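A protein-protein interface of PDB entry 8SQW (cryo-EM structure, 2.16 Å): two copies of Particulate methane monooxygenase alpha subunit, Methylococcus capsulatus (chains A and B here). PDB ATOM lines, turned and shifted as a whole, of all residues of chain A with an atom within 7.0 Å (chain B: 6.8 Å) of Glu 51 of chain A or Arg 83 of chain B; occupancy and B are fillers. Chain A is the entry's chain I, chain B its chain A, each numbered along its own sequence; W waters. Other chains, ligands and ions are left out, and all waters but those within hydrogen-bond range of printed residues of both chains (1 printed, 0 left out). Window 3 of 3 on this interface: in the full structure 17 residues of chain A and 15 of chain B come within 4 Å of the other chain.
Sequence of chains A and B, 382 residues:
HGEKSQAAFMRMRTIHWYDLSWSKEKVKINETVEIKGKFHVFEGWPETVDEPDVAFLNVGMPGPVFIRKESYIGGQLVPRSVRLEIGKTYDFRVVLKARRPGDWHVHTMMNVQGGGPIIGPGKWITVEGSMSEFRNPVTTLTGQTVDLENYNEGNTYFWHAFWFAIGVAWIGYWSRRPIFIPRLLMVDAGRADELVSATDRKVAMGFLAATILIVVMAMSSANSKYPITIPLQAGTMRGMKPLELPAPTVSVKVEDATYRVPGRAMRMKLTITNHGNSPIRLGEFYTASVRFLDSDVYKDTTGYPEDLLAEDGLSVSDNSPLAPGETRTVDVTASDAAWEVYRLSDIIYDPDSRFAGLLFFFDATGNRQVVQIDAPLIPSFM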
ATOM      1  N   GLU A  43      15.823  -3.168  12.174  1.00  0.00           N
ATOM      2  CA  GLU A  43      16.226  -2.016  11.377  1.00  0.00           C
ATOM      3  C   GLU A  43      15.067  -1.477  10.548  1.00  0.00           C
ATOM      4  O   GLU A  43      14.903  -0.258  10.413  1.00  0.00           O
ATOM      5  CB  GLU A  43      17.401  -2.387  10.473  1.00  0.00           C
ATOM      6  CG  GLU A  43      18.726  -2.507  11.203  1.00  0.00           C
ATOM      7  CD  GLU A  43      18.926  -3.874  11.826  1.00  0.00           C
ATOM      8  OE1 GLU A  43      18.004  -4.709  11.735  1.00  0.00           O
ATOM      9  OE2 GLU A  43      20.006  -4.111  12.407  1.00  0.00           O
ATOM     10  N   TRP A  45      12.120  -0.718  11.016  1.00  0.00           N
ATOM     11  CA  TRP A  45      11.058  -0.308  11.924  1.00  0.00           C
ATOM     12  C   TRP A  45       9.915   0.321  11.131  1.00  0.00           C
ATOM     13  O   TRP A  45      10.154   1.246  10.341  1.00  0.00           O
ATOM     14  CB  TRP A  45      11.620   0.688  12.933  1.00  0.00           C
ATOM     15  CG  TRP A  45      10.731   1.020  14.082  1.00  0.00           C
ATOM     16  CD1 TRP A  45       9.887   2.084  14.181  1.00  0.00           C
ATOM     17  CD2 TRP A  45      10.643   0.317  15.325  1.00  0.00           C
ATOM     18  NE1 TRP A  45       9.256   2.073  15.399  1.00  0.00           N
ATOM     19  CE2 TRP A  45       9.705   0.999  16.122  1.00  0.00           C
ATOM     20  CE3 TRP A  45      11.254  -0.829  15.837  1.00  0.00           C
ATOM     21  CZ2 TRP A  45       9.363   0.572  17.403  1.00  0.00           C
ATOM     22  CZ3 TRP A  45      10.912  -1.248  17.109  1.00  0.00           C
ATOM     23  CH2 TRP A  45       9.976  -0.551  17.874  1.00  0.00           C
ATOM     24  N   PRO A  46       8.680  -0.146  11.299  1.00  0.00           N
ATOM     25  CA  PRO A  46       7.575   0.380  10.486  1.00  0.00           C
ATOM     26  C   PRO A  46       7.368   1.869  10.726  1.00  0.00           C
ATOM     27  O   PRO A  46       7.474   2.353  11.855  1.00  0.00           O
ATOM     28  CB  PRO A  46       6.369  -0.445  10.946  1.00  0.00           C
ATOM     29  CG  PRO A  46       6.745  -0.960  12.292  1.00  0.00           C
ATOM     30  CD  PRO A  46       8.228  -1.147  12.279  1.00  0.00           C
ATOM     31  N   GLU A  47       7.071   2.593   9.646  1.00  0.00           N
ATOM     32  CA  GLU A  47       6.889   4.037   9.750  1.00  0.00           C
ATOM     33  C   GLU A  47       5.666   4.404  10.576  1.00  0.00           C
ATOM     34  O   GLU A  47       5.622   5.498  11.149  1.00  0.00           O
ATOM     35  CB  GLU A  47       6.782   4.654   8.354  1.00  0.00           C
ATOM     36  CG  GLU A  47       5.438   4.447   7.674  1.00  0.00           C
ATOM     37  CD  GLU A  47       5.042   5.622   6.803  1.00  0.00           C
ATOM     38  OE1 GLU A  47       5.411   6.765   7.139  1.00  0.00           O
ATOM     39  OE2 GLU A  47       4.366   5.401   5.777  1.00  0.00           O
ATOM     40  N   VAL A  49       4.854   3.095  13.356  1.00  0.00           N
ATOM     41  CA  VAL A  49       5.294   3.094  14.742  1.00  0.00           C
ATOM     42  C   VAL A  49       6.370   4.152  14.902  1.00  0.00           C
ATOM     43  O   VAL A  49       7.353   4.187  14.154  1.00  0.00           O
ATOM     44  CB  VAL A  49       5.821   1.707  15.172  1.00  0.00           C
ATOM     45  CG1 VAL A  49       6.206   1.718  16.634  1.00  0.00           C
ATOM     46  CG2 VAL A  49       4.781   0.655  14.911  1.00  0.00           C
ATOM     47  N   ASP A  50       6.180   5.031  15.879  1.00  0.00           N
ATOM     48  CA  ASP A  50       7.204   6.017  16.176  1.00  0.00           C
ATOM     49  C   ASP A  50       8.489   5.317  16.601  1.00  0.00           C
ATOM     50  O   ASP A  50       8.472   4.233  17.188  1.00  0.00           O
ATOM     51  CB  ASP A  50       6.739   6.974  17.275  1.00  0.00           C
ATOM     52  CG  ASP A  50       5.843   8.079  16.746  1.00  0.00           C
ATOM     53  OD1 ASP A  50       5.332   7.948  15.615  1.00  0.00           O
ATOM     54  OD2 ASP A  50       5.653   9.082  17.466  1.00  0.00           O
ATOM     55  N   GLU A  51       9.613   5.945  16.276  1.00  0.00           N
ATOM     56  CA  GLU A  51      10.902   5.383  16.630  1.00  0.00           C
ATOM     57  C   GLU A  51      11.001   5.234  18.148  1.00  0.00           C
ATOM     58  O   GLU A  51      10.480   6.064  18.896  1.00  0.00           O
ATOM     59  CB  GLU A  51      12.030   6.268  16.113  1.00  0.00           C
ATOM     60  CG  GLU A  51      12.541   5.856  14.747  1.00  0.00           C
ATOM     61  CD  GLU A  51      13.085   7.018  13.945  1.00  0.00           C
ATOM     62  OE1 GLU A  51      12.290   7.899  13.562  1.00  0.00           O
ATOM     63  OE2 GLU A  51      14.309   7.046  13.695  1.00  0.00           O
ATOM     64  N   PRO A  52      11.661   4.179  18.629  1.00  0.00           N
ATOM     65  CA  PRO A  52      11.686   3.936  20.078  1.00  0.00           C
ATOM     66  C   PRO A  52      12.564   4.925  20.828  1.00  0.00           C
ATOM     67  O   PRO A  52      13.419   4.532  21.627  1.00  0.00           O
ATOM     68  CB  PRO A  52      12.232   2.506  20.180  1.00  0.00           C
ATOM     69  CG  PRO A  52      13.039   2.324  18.945  1.00  0.00           C
ATOM     70  CD  PRO A  52      12.360   3.126  17.874  1.00  0.00           C
ATOM     71  N   ASP A  53      12.354   6.219  20.571  1.00  0.00           N
ATOM     72  CA  ASP A  53      13.056   7.254  21.321  1.00  0.00           C
ATOM     73  C   ASP A  53      12.640   7.253  22.784  1.00  0.00           C
ATOM     74  O   ASP A  53      13.458   7.554  23.661  1.00  0.00           O
ATOM     75  CB  ASP A  53      12.793   8.621  20.696  1.00  0.00           C
ATOM     76  CG  ASP A  53      13.505   8.800  19.371  1.00  0.00           C
ATOM     77  OD1 ASP A  53      14.333   7.938  19.016  1.00  0.00           O
ATOM     78  OD2 ASP A  53      13.231   9.807  18.686  1.00  0.00           O
ATOM     79  N   VAL A  54      11.379   6.943  23.064  1.00  0.00           N
ATOM     80  CA  VAL A  54      10.867   6.845  24.427  1.00  0.00           C
ATOM     81  C   VAL A  54      10.192   5.484  24.532  1.00  0.00           C
ATOM     82  O   VAL A  54       9.127   5.263  23.945  1.00  0.00           O
ATOM     83  CB  VAL A  54       9.891   7.976  24.769  1.00  0.00           C
ATOM     84  CG1 VAL A  54       9.419   7.839  26.194  1.00  0.00           C
ATOM     85  CG2 VAL A  54      10.548   9.334  24.555  1.00  0.00           C
ATOM     86  N   ALA A  55      10.808   4.565  25.271  1.00  0.00           N
ATOM     87  CA  ALA A  55      10.300   3.212  25.425  1.00  0.00           C
ATOM     88  C   ALA A  55      10.360   2.804  26.887  1.00  0.00           C
ATOM     89  O   ALA A  55      11.229   3.253  27.637  1.00  0.00           O
ATOM     90  CB  ALA A  55      11.086   2.213  24.568  1.00  0.00           C
ATOM     91  N   LEU A  84      15.819   3.751  23.097  1.00  0.00           N
ATOM     92  CA  LEU A  84      16.412   2.626  22.397  1.00  0.00           C
ATOM     93  C   LEU A  84      16.813   3.054  20.993  1.00  0.00           C
ATOM     94  O   LEU A  84      16.191   3.943  20.407  1.00  0.00           O
ATOM     95  CB  LEU A  84      15.444   1.442  22.334  1.00  0.00           C
ATOM     96  CG  LEU A  84      15.001   0.880  23.686  1.00  0.00           C
ATOM     97  CD1 LEU A  84      13.933  -0.183  23.499  1.00  0.00           C
ATOM     98  CD2 LEU A  84      16.189   0.328  24.453  1.00  0.00           C
ATOM     99  N   ILE A  86      17.492   1.986  16.998  1.00  0.00           N
ATOM    100  CA  ILE A  86      17.095   1.011  15.990  1.00  0.00           C
ATOM    101  C   ILE A  86      18.324   0.261  15.496  1.00  0.00           C
ATOM    102  O   ILE A  86      19.358   0.865  15.188  1.00  0.00           O
ATOM    103  CB  ILE A  86      16.360   1.711  14.836  1.00  0.00           C
ATOM    104  CG1 ILE A  86      14.983   2.181  15.294  1.00  0.00           C
ATOM    105  CG2 ILE A  86      16.230   0.792  13.639  1.00  0.00           C
ATOM    106  CD1 ILE A  86      14.171   2.796  14.194  1.00  0.00           C
ATOM    107  N   VAL A 112       6.223   1.466  23.356  1.00  0.00           N
ATOM    108  CA  VAL A 112       6.881   2.539  22.622  1.00  0.00           C
ATOM    109  C   VAL A 112       5.962   3.751  22.614  1.00  0.00           C
ATOM    110  O   VAL A 112       4.746   3.618  22.432  1.00  0.00           O
ATOM    111  CB  VAL A 112       7.244   2.098  21.193  1.00  0.00           C
ATOM    112  CG1 VAL A 112       7.888   3.235  20.424  1.00  0.00           C
ATOM    113  CG2 VAL A 112       8.177   0.905  21.246  1.00  0.00           C
ATOM    114  N   GLN A 113       6.547   4.933  22.827  1.00  0.00           N
ATOM    115  CA  GLN A 113       5.775   6.154  23.042  1.00  0.00           C
ATOM    116  C   GLN A 113       4.722   6.387  21.967  1.00  0.00           C
ATOM    117  O   GLN A 113       3.573   6.713  22.272  1.00  0.00           O
ATOM    118  CB  GLN A 113       6.723   7.352  23.121  1.00  0.00           C
ATOM    119  CG  GLN A 113       6.036   8.704  23.027  1.00  0.00           C
ATOM    120  CD  GLN A 113       5.608   9.239  24.375  1.00  0.00           C
ATOM    121  OE1 GLN A 113       4.535   8.905  24.877  1.00  0.00           O
ATOM    122  NE2 GLN A 113       6.444  10.076  24.973  1.00  0.00           N
ATOM    123  N   GLY A 114       5.086   6.220  20.700  1.00  0.00           N
ATOM    124  CA  GLY A 114       4.132   6.490  19.645  1.00  0.00           C
ATOM    125  C   GLY A 114       3.757   5.290  18.803  1.00  0.00           C
ATOM    126  O   GLY A 114       3.350   5.447  17.649  1.00  0.00           O
ATOM    127  N   GLY A 115       3.899   4.086  19.348  1.00  0.00           N
ATOM    128  CA  GLY A 115       3.520   2.914  18.590  1.00  0.00           C
ATOM    129  C   GLY A 115       2.688   1.887  19.330  1.00  0.00           C
ATOM    130  O   GLY A 115       2.092   1.015  18.701  1.00  0.00           O
ATOM    131  N   PRO B  52      15.119  13.821   4.861  1.00  0.00           N
ATOM    132  CA  PRO B  52      14.524  12.824   3.958  1.00  0.00           C
ATOM    133  C   PRO B  52      14.231  11.503   4.650  1.00  0.00           C
ATOM    134  O   PRO B  52      14.613  10.435   4.163  1.00  0.00           O
ATOM    135  CB  PRO B  52      15.589  12.665   2.867  1.00  0.00           C
ATOM    136  CG  PRO B  52      16.867  13.031   3.532  1.00  0.00           C
ATOM    137  CD  PRO B  52      16.531  14.091   4.539  1.00  0.00           C
ATOM    138  N   ASP B  53      13.544  11.570   5.794  1.00  0.00           N
ATOM    139  CA  ASP B  53      13.106  10.359   6.477  1.00  0.00           C
ATOM    140  C   ASP B  53      12.075   9.604   5.652  1.00  0.00           C
ATOM    141  O   ASP B  53      12.032   8.370   5.694  1.00  0.00           O
ATOM    142  CB  ASP B  53      12.535  10.709   7.849  1.00  0.00           C
ATOM    143  CG  ASP B  53      13.605  11.132   8.834  1.00  0.00           C
ATOM    144  OD1 ASP B  53      14.803  10.993   8.512  1.00  0.00           O
ATOM    145  OD2 ASP B  53      13.244  11.604   9.931  1.00  0.00           O
ATOM    146  N   VAL B  54      11.228  10.321   4.921  1.00  0.00           N
ATOM    147  CA  VAL B  54      10.234   9.722   4.038  1.00  0.00           C
ATOM    148  C   VAL B  54      10.425  10.373   2.676  1.00  0.00           C
ATOM    149  O   VAL B  54      10.109  11.553   2.493  1.00  0.00           O
ATOM    150  CB  VAL B  54       8.802   9.915   4.551  1.00  0.00           C
ATOM    151  CG1 VAL B  54       7.823   9.252   3.616  1.00  0.00           C
ATOM    152  CG2 VAL B  54       8.657   9.355   5.960  1.00  0.00           C
ATOM    153  N   ALA B  55      10.948   9.612   1.718  1.00  0.00           N
ATOM    154  CA  ALA B  55      11.224  10.116   0.381  1.00  0.00           C
ATOM    155  C   ALA B  55      10.731   9.119  -0.654  1.00  0.00           C
ATOM    156  O   ALA B  55      10.712   7.909  -0.415  1.00  0.00           O
ATOM    157  CB  ALA B  55      12.718  10.388   0.178  1.00  0.00           C
ATOM    158  N   ILE B  73      16.239   1.741  -5.694  1.00  0.00           N
ATOM    159  CA  ILE B  73      17.248   2.474  -4.942  1.00  0.00           C
ATOM    160  C   ILE B  73      18.192   1.436  -4.354  1.00  0.00           C
ATOM    161  O   ILE B  73      17.764   0.564  -3.586  1.00  0.00           O
ATOM    162  CB  ILE B  73      16.627   3.352  -3.846  1.00  0.00           C
ATOM    163  CG1 ILE B  73      15.742   4.433  -4.471  1.00  0.00           C
ATOM    164  CG2 ILE B  73      17.719   3.965  -2.978  1.00  0.00           C
ATOM    165  CD1 ILE B  73      15.452   5.599  -3.553  1.00  0.00           C
ATOM    166  N   SER B  81       7.336   4.804  -0.490  1.00  0.00           N
ATOM    167  CA  SER B  81       8.275   5.791   0.020  1.00  0.00           C
ATOM    168  C   SER B  81       9.418   5.099   0.753  1.00  0.00           C
ATOM    169  O   SER B  81       9.269   3.996   1.280  1.00  0.00           O
ATOM    170  CB  SER B  81       7.566   6.771   0.950  1.00  0.00           C
ATOM    171  OG  SER B  81       6.798   6.086   1.922  1.00  0.00           O
ATOM    172  N   VAL B  82      10.576   5.753   0.764  1.00  0.00           N
ATOM    173  CA  VAL B  82      11.776   5.176   1.350  1.00  0.00           C
ATOM    174  C   VAL B  82      12.419   6.191   2.282  1.00  0.00           C
ATOM    175  O   VAL B  82      12.142   7.390   2.228  1.00  0.00           O
ATOM    176  CB  VAL B  82      12.786   4.715   0.282  1.00  0.00           C
ATOM    177  CG1 VAL B  82      12.133   3.740  -0.673  1.00  0.00           C
ATOM    178  CG2 VAL B  82      13.351   5.907  -0.468  1.00  0.00           C
ATOM    179  N   ARG B  83      13.291   5.688   3.146  1.00  0.00           N
ATOM    180  CA  ARG B  83      14.046   6.518   4.072  1.00  0.00           C
ATOM    181  C   ARG B  83      15.467   6.677   3.552  1.00  0.00           C
ATOM    182  O   ARG B  83      16.142   5.688   3.260  1.00  0.00           O
ATOM    183  CB  ARG B  83      14.061   5.906   5.470  1.00  0.00           C
ATOM    184  CG  ARG B  83      15.094   6.520   6.398  1.00  0.00           C
ATOM    185  CD  ARG B  83      15.046   5.879   7.770  1.00  0.00           C
ATOM    186  NE  ARG B  83      14.114   6.571   8.652  1.00  0.00           N
ATOM    187  CZ  ARG B  83      14.470   7.451   9.576  1.00  0.00           C
ATOM    188  NH1 ARG B  83      15.739   7.773   9.775  1.00  0.00           N
ATOM    189  NH2 ARG B  83      13.529   8.024  10.320  1.00  0.00           N
ATOM    190  N   LEU B  84      15.914   7.923   3.439  1.00  0.00           N
ATOM    191  CA  LEU B  84      17.263   8.240   3.002  1.00  0.00           C
ATOM    192  C   LEU B  84      18.031   8.878   4.149  1.00  0.00           C
ATOM    193  O   LEU B  84      17.441   9.539   5.009  1.00  0.00           O
ATOM    194  CB  LEU B  84      17.246   9.174   1.791  1.00  0.00           C
ATOM    195  CG  LEU B  84      16.545   8.627   0.547  1.00  0.00           C
ATOM    196  CD1 LEU B  84      16.460   9.694  -0.532  1.00  0.00           C
ATOM    197  CD2 LEU B  84      17.255   7.389   0.030  1.00  0.00           C
ATOM    198  N   GLU B  85      19.343   8.677   4.161  1.00  0.00           N
ATOM    199  CA  GLU B  85      20.210   9.213   5.198  1.00  0.00           C
ATOM    200  C   GLU B  85      21.028  10.366   4.635  1.00  0.00           C
ATOM    201  O   GLU B  85      21.585  10.265   3.537  1.00  0.00           O
ATOM    202  CB  GLU B  85      21.128   8.130   5.761  1.00  0.00           C
ATOM    203  CG  GLU B  85      20.400   6.932   6.365  1.00  0.00           C
ATOM    204  CD  GLU B  85      19.355   7.314   7.405  1.00  0.00           C
ATOM    205  OE1 GLU B  85      19.529   8.343   8.090  1.00  0.00           O
ATOM    206  OE2 GLU B  85      18.356   6.575   7.536  1.00  0.00           O
ATOM    207  N   TYR B  90      23.411   7.139  -2.971  1.00  0.00           N
ATOM    208  CA  TYR B  90      22.641   5.994  -3.423  1.00  0.00           C
ATOM    209  C   TYR B  90      22.654   5.944  -4.940  1.00  0.00           C
ATOM    210  O   TYR B  90      22.716   6.977  -5.612  1.00  0.00           O
ATOM    211  CB  TYR B  90      21.186   6.047  -2.932  1.00  0.00           C
ATOM    212  CG  TYR B  90      21.023   6.219  -1.442  1.00  0.00           C
ATOM    213  CD1 TYR B  90      21.093   7.475  -0.855  1.00  0.00           C
ATOM    214  CD2 TYR B  90      20.790   5.126  -0.617  1.00  0.00           C
ATOM    215  CE1 TYR B  90      20.942   7.637   0.503  1.00  0.00           C
ATOM    216  CE2 TYR B  90      20.636   5.280   0.744  1.00  0.00           C
ATOM    217  CZ  TYR B  90      20.713   6.536   1.299  1.00  0.00           C
ATOM    218  OH  TYR B  90      20.561   6.698   2.654  1.00  0.00           O
ATOM    219  N   THR B 236       6.347   3.371   4.425  1.00  0.00           N
ATOM    220  CA  THR B 236       7.721   3.734   4.105  1.00  0.00           C
ATOM    221  C   THR B 236       8.648   2.545   4.321  1.00  0.00           C
ATOM    222  O   THR B 236       8.518   1.802   5.299  1.00  0.00           O
ATOM    223  CB  THR B 236       8.171   4.920   4.961  1.00  0.00           C
ATOM    224  OG1 THR B 236       7.291   6.030   4.740  1.00  0.00           O
ATOM    225  CG2 THR B 236       9.591   5.337   4.609  1.00  0.00           C
ATOM    226  N   MET B 237       9.584   2.364   3.397  1.00  0.00           N
ATOM    227  CA  MET B 237      10.499   1.232   3.416  1.00  0.00           C
ATOM    228  C   MET B 237      11.857   1.697   3.926  1.00  0.00           C
ATOM    229  O   MET B 237      12.462   2.610   3.352  1.00  0.00           O
ATOM    230  CB  MET B 237      10.620   0.622   2.023  1.00  0.00           C
ATOM    231  CG  MET B 237       9.402  -0.190   1.613  1.00  0.00           C
ATOM    232  SD  MET B 237       9.411  -0.636  -0.131  1.00  0.00           S
ATOM    233  CE  MET B 237      11.015  -1.409  -0.258  1.00  0.00           C
ATOM    234  N   ARG B 238      12.329   1.073   4.998  1.00  0.00           N
ATOM    235  CA  ARG B 238      13.606   1.406   5.603  1.00  0.00           C
ATOM    236  C   ARG B 238      14.705   0.520   5.027  1.00  0.00           C
ATOM    237  O   ARG B 238      14.466  -0.361   4.194  1.00  0.00           O
ATOM    238  CB  ARG B 238      13.533   1.260   7.122  1.00  0.00           C
ATOM    239  CG  ARG B 238      13.445   2.569   7.878  1.00  0.00           C
ATOM    240  CD  ARG B 238      12.900   2.343   9.278  1.00  0.00           C
ATOM    241  NE  ARG B 238      13.110   3.489  10.152  1.00  0.00           N
ATOM    242  CZ  ARG B 238      14.273   3.815  10.700  1.00  0.00           C
ATOM    243  NH1 ARG B 238      15.360   3.090  10.491  1.00  0.00           N
ATOM    244  NH2 ARG B 238      14.344   4.888  11.478  1.00  0.00           N
ATOM    245  N   GLY B 239      15.928   0.755   5.486  1.00  0.00           N
ATOM    246  CA  GLY B 239      17.058  -0.059   5.092  1.00  0.00           C
ATOM    247  C   GLY B 239      17.424   0.033   3.626  1.00  0.00           C
ATOM    248  O   GLY B 239      17.710  -0.986   2.990  1.00  0.00           O
ATOM    249  N   MET B 240      17.409   1.243   3.071  1.00  0.00           N
ATOM    250  CA  MET B 240      17.953   1.474   1.737  1.00  0.00           C
ATOM    251  C   MET B 240      19.466   1.326   1.812  1.00  0.00           C
ATOM    252  O   MET B 240      20.109   1.905   2.691  1.00  0.00           O
ATOM    253  CB  MET B 240      17.558   2.852   1.217  1.00  0.00           C
ATOM    254  CG  MET B 240      16.059   3.086   1.079  1.00  0.00           C
ATOM    255  SD  MET B 240      15.270   2.052  -0.174  1.00  0.00           S
ATOM    256  CE  MET B 240      14.650   0.691   0.815  1.00  0.00           C
HETATM  257  O   HOH W   1       6.940   0.627   7.235  1.00  0.00           O
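The side-chain carboxylate (OE1) of Glu 47 of chain A lies close to the side-chain hydroxyl (OG1) of Thr 236 of chain B (3.1 Å).
The guanidinium group (NH1) of Arg 238 of chain B is in hydrogen-bond range of the backbone carbonyl oxygen (O) of Glu 43 of chain A.
The guanidinium group (NH2) of Arg 83 of chain B is in salt-bridge range of the side-chain carboxylate (OE1) of Glu 51 of chain A (3.5 Å).
NH2 of Arg 238 of chain B is in salt-bridge range of OE2 of Glu 51 of chain A.
The side-chain carboxylate of Glu 85 of chain B is in salt-bridge range of the guanidinium group of Arg 83 of chain B, at 3.6 Å.
The backbone NH (N) of Arg 83 of chain B sits at hydrogen-bond distance from the backbone carbonyl oxygen (O) of Met 237 of chain B, at 3.2 Å.
OG of Ser 81 of chain B is in hydrogen-bond range of OG1 of Thr 236 of chain B.
The backbone carbonyl oxygen of Val 49 of chain A sits at hydrogen-bond distance from the indole nitrogen of Trp 45 of chain A, 3.1 Å away.
OD1 of Asp 53 of chain B lies within salt-bridge range of NH1 of Arg 83 of chain B (3.6 Å).
The indole nitrogen of Trp 45 of chain A sits at hydrogen-bond distance from the backbone carbonyl oxygen of Asp 50 of chain A (2.9 Å).
CD of Arg 238 of chain B touches O of Trp 45 of chain A (3.1 Å).
CD1 of Ile 86 of chain A touches NH2 of Arg 238 of chain B, 3.4 Å away.
Of the printed residues of chain B, Glu 43 of chain A touches Arg 238 (3.4 Å).
Printed residues of chain B within 4 Å of Trp 45 of chain A: Arg 238 (3.1 Å).
Of the printed residues of chain B, Glu 47 of chain A touches Thr 236 (3.1 Å).
Of chain B, only Arg 83 and Arg 238 come within 4 Å of Glu 51 of chain A.
Printed residues of chain B within 4 Å of Ile 86 of chain A: Arg 238 (3.4 Å).
Printed residues of chain A within 4 Å of Arg 238 of chain B: Glu 43, Trp 45, Glu 51 and Ile 86.
The nearest residue of chain B that does not touch Glu 51 of chain A is Asp 53 of chain B (5.3 Å).
The nearest residue of chain A that does not touch Arg 83 of chain B is Ile 86 of chain A (6.5 Å).
Printed residues of chain A that touch a printed residue of chain B: Glu 43, Trp 45, Glu 47, Glu 51 and Ile 86.
Of the 16 printed residues of chain B, 3 touch a printed residue of chain A.
Positions printed for both chains: 52, 53, 54, 55 and 84.
Of the 6 pairs that touch across the chains among the printed residues, none has its exchanged pair printed and touching as well.
Water W1 lies within hydrogen-bond range of the backbone carbonyl oxygen of Thr 236 of chain B and the backbone NH of Glu 47 of chain A.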
